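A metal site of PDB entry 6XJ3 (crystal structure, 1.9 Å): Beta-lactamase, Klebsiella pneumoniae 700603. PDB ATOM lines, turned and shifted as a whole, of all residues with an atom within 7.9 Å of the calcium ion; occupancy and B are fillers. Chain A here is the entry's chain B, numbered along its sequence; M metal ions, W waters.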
ATOM      1  N   ASP A  30     -22.719   2.169  -0.742  1.00  0.00           N
ATOM      2  CA  ASP A  30     -22.215   2.622   0.549  1.00  0.00           C
ATOM      3  C   ASP A  30     -20.702   2.461   0.567  1.00  0.00           C
ATOM      4  O   ASP A  30     -20.199   1.336   0.644  1.00  0.00           O
ATOM      5  CB  ASP A  30     -22.873   1.837   1.690  1.00  0.00           C
ATOM      6  CG  ASP A  30     -22.445   2.302   3.078  1.00  0.00           C
ATOM      7  OD1 ASP A  30     -21.595   3.211   3.255  1.00  0.00           O
ATOM      8  OD2 ASP A  30     -22.994   1.736   4.031  1.00  0.00           O
ATOM      9  N   GLU A  31     -19.973   3.571   0.496  1.00  0.00           N
ATOM     10  CA  GLU A  31     -18.528   3.546   0.520  1.00  0.00           C
ATOM     11  C   GLU A  31     -17.929   3.767   1.903  1.00  0.00           C
ATOM     12  O   GLU A  31     -16.724   3.994   2.007  1.00  0.00           O
ATOM     13  CB  GLU A  31     -17.961   4.587  -0.441  1.00  0.00           C
ATOM     14  CG  GLU A  31     -18.420   4.419  -1.843  1.00  0.00           C
ATOM     15  CD  GLU A  31     -17.609   5.224  -2.853  1.00  0.00           C
ATOM     16  OE1 GLU A  31     -16.884   6.175  -2.457  1.00  0.00           O
ATOM     17  OE2 GLU A  31     -17.718   4.898  -4.046  1.00  0.00           O
ATOM     18  N   ARG A  32     -18.729   3.742   2.965  1.00  0.00           N
ATOM     19  CA  ARG A  32     -18.154   3.969   4.276  1.00  0.00           C
ATOM     20  C   ARG A  32     -17.309   2.772   4.688  1.00  0.00           C
ATOM     21  O   ARG A  32     -17.729   1.621   4.537  1.00  0.00           O
ATOM     22  CB  ARG A  32     -19.238   4.222   5.308  1.00  0.00           C
ATOM     23  CG  ARG A  32     -19.968   5.539   5.116  1.00  0.00           C
ATOM     24  CD  ARG A  32     -21.191   5.590   6.025  1.00  0.00           C
ATOM     25  NE  ARG A  32     -22.149   4.524   5.718  1.00  0.00           N
ATOM     26  CZ  ARG A  32     -23.252   4.294   6.429  1.00  0.00           C
ATOM     27  NH1 ARG A  32     -23.533   5.046   7.478  1.00  0.00           N
ATOM     28  NH2 ARG A  32     -24.068   3.298   6.082  1.00  0.00           N
ATOM     29  N   GLN A  33     -16.121   3.052   5.233  1.00  0.00           N
ATOM     30  CA  GLN A  33     -15.142   2.046   5.658  1.00  0.00           C
ATOM     31  C   GLN A  33     -15.065   0.977   4.570  1.00  0.00           C
ATOM     32  O   GLN A  33     -14.879   1.323   3.397  1.00  0.00           O
ATOM     33  CB  GLN A  33     -15.495   1.556   7.049  1.00  0.00           C
ATOM     34  CG  GLN A  33     -15.510   2.684   8.080  1.00  0.00           C
ATOM     35  CD  GLN A  33     -15.812   2.217   9.503  1.00  0.00           C
ATOM     36  OE1 GLN A  33     -16.751   1.452   9.735  1.00  0.00           O
ATOM     37  NE2 GLN A  33     -15.020   2.684  10.459  1.00  0.00           N
ATOM     38  N   ALA A  34     -15.205  -0.306   4.900  1.00  0.00           N
ATOM     39  CA  ALA A  34     -15.263  -1.325   3.854  1.00  0.00           C
ATOM     40  C   ALA A  34     -16.488  -1.090   2.988  1.00  0.00           C
ATOM     41  O   ALA A  34     -17.614  -1.006   3.499  1.00  0.00           O
ATOM     42  CB  ALA A  34     -15.297  -2.723   4.474  1.00  0.00           C
ATOM     43  N   ASP A  35     -16.267  -0.953   1.690  1.00  0.00           N
ATOM     44  CA  ASP A  35     -17.379  -0.788   0.775  1.00  0.00           C
ATOM     45  C   ASP A  35     -18.257  -2.035   0.803  1.00  0.00           C
ATOM     46  O   ASP A  35     -17.771  -3.166   0.708  1.00  0.00           O
ATOM     47  CB  ASP A  35     -16.876  -0.515  -0.647  1.00  0.00           C
ATOM     48  CG  ASP A  35     -16.080   0.773  -0.749  1.00  0.00           C
ATOM     49  OD1 ASP A  35     -15.835   1.418   0.296  1.00  0.00           O
ATOM     50  OD2 ASP A  35     -15.705   1.135  -1.894  1.00  0.00           O
ATOM     51  N   ARG A  36     -19.562  -1.819   0.967  1.00  0.00           N
ATOM     52  CA  ARG A  36     -20.517  -2.908   0.790  1.00  0.00           C
ATOM     53  C   ARG A  36     -20.551  -3.308  -0.681  1.00  0.00           C
ATOM     54  O   ARG A  36     -20.033  -2.619  -1.561  1.00  0.00           O
ATOM     55  CB  ARG A  36     -21.934  -2.486   1.210  1.00  0.00           C
ATOM     56  CG  ARG A  36     -22.123  -2.009   2.653  1.00  0.00           C
ATOM     57  CD  ARG A  36     -23.600  -1.631   2.912  1.00  0.00           C
ATOM     58  NE  ARG A  36     -23.739  -0.899   4.166  1.00  0.00           N
ATOM     59  CZ  ARG A  36     -24.622  -1.180   5.128  1.00  0.00           C
ATOM     60  NH1 ARG A  36     -25.486  -2.175   4.990  1.00  0.00           N
ATOM     61  NH2 ARG A  36     -24.641  -0.437   6.235  1.00  0.00           N
ATOM     62  N   ARG A 162     -15.802  12.295  -7.168  1.00  0.00           N
ATOM     63  CA  ARG A 162     -14.353  12.128  -7.243  1.00  0.00           C
ATOM     64  C   ARG A 162     -13.665  13.199  -8.087  1.00  0.00           C
ATOM     65  O   ARG A 162     -12.450  13.103  -8.278  1.00  0.00           O
ATOM     66  CB  ARG A 162     -13.996  10.744  -7.789  1.00  0.00           C
ATOM     67  CG  ARG A 162     -14.449   9.577  -6.924  1.00  0.00           C
ATOM     68  CD  ARG A 162     -13.542   9.362  -5.716  1.00  0.00           C
ATOM     69  NE  ARG A 162     -14.105   8.366  -4.809  1.00  0.00           N
ATOM     70  CZ  ARG A 162     -13.567   8.015  -3.641  1.00  0.00           C
ATOM     71  NH1 ARG A 162     -12.430   8.572  -3.248  1.00  0.00           N
ATOM     72  NH2 ARG A 162     -14.166   7.116  -2.878  1.00  0.00           N
ATOM     73  N   THR A 210     -16.338   8.699   7.269  1.00  0.00           N
ATOM     74  CA  THR A 210     -15.705   7.480   6.770  1.00  0.00           C
ATOM     75  C   THR A 210     -16.010   7.200   5.306  1.00  0.00           C
ATOM     76  O   THR A 210     -15.558   6.187   4.773  1.00  0.00           O
ATOM     77  CB  THR A 210     -16.123   6.284   7.632  1.00  0.00           C
ATOM     78  OG1 THR A 210     -17.557   6.195   7.689  1.00  0.00           O
ATOM     79  CG2 THR A 210     -15.590   6.443   9.041  1.00  0.00           C
ATOM     80  N   GLY A 211     -16.754   8.090   4.636  1.00  0.00           N
ATOM     81  CA  GLY A 211     -17.009   7.918   3.219  1.00  0.00           C
ATOM     82  C   GLY A 211     -18.424   8.276   2.885  1.00  0.00           C
ATOM     83  O   GLY A 211     -19.213   8.677   3.768  1.00  0.00           O
ATOM     84  N   SER A 212     -18.805   8.133   1.631  1.00  0.00           N
ATOM     85  CA  SER A 212     -20.108   8.595   1.197  1.00  0.00           C
ATOM     86  C   SER A 212     -21.008   7.438   0.792  1.00  0.00           C
ATOM     87  O   SER A 212     -20.555   6.336   0.480  1.00  0.00           O
ATOM     88  CB  SER A 212     -19.941   9.607   0.071  1.00  0.00           C
ATOM     89  OG  SER A 212     -19.142  10.673   0.587  1.00  0.00           O
HETATM   90 CA    CA M   1     -14.468   3.052   1.771  1.00  0.00          CA
HETATM   91  O   HOH W   1     -14.085   4.285  -0.224  1.00  0.00           O
HETATM   92  O   HOH W   2     -14.194   5.328   2.389  1.00  0.00           O
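The backbone carbonyl oxygen (O) of Ser 212 sits at hydrogen-bond distance from the backbone NH (N) of Glu 31 (2.8 Å).
OE1 of Glu 31 is in salt-bridge range of NH2 of Arg 162 (2.9 Å).
The backbone carbonyl oxygen (O) of Thr 210 is in hydrogen-bond range of the backbone NH (N) of Gln 33 (3.2 Å).
The calcium ion is bound by water W2 (2.4 Å).
The calcium ion is bound by water W1 (2.4 Å).
The calcium ion is bound by O of Gln 33, at 2.4 Å.
O of Glu 31 binds the calcium ion (2.5 Å).
OD1 of Asp 35 is bound to the calcium ion (2.6 Å).
Of the 11 residues printed, 3 come within 4 Å of the calcium ion.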
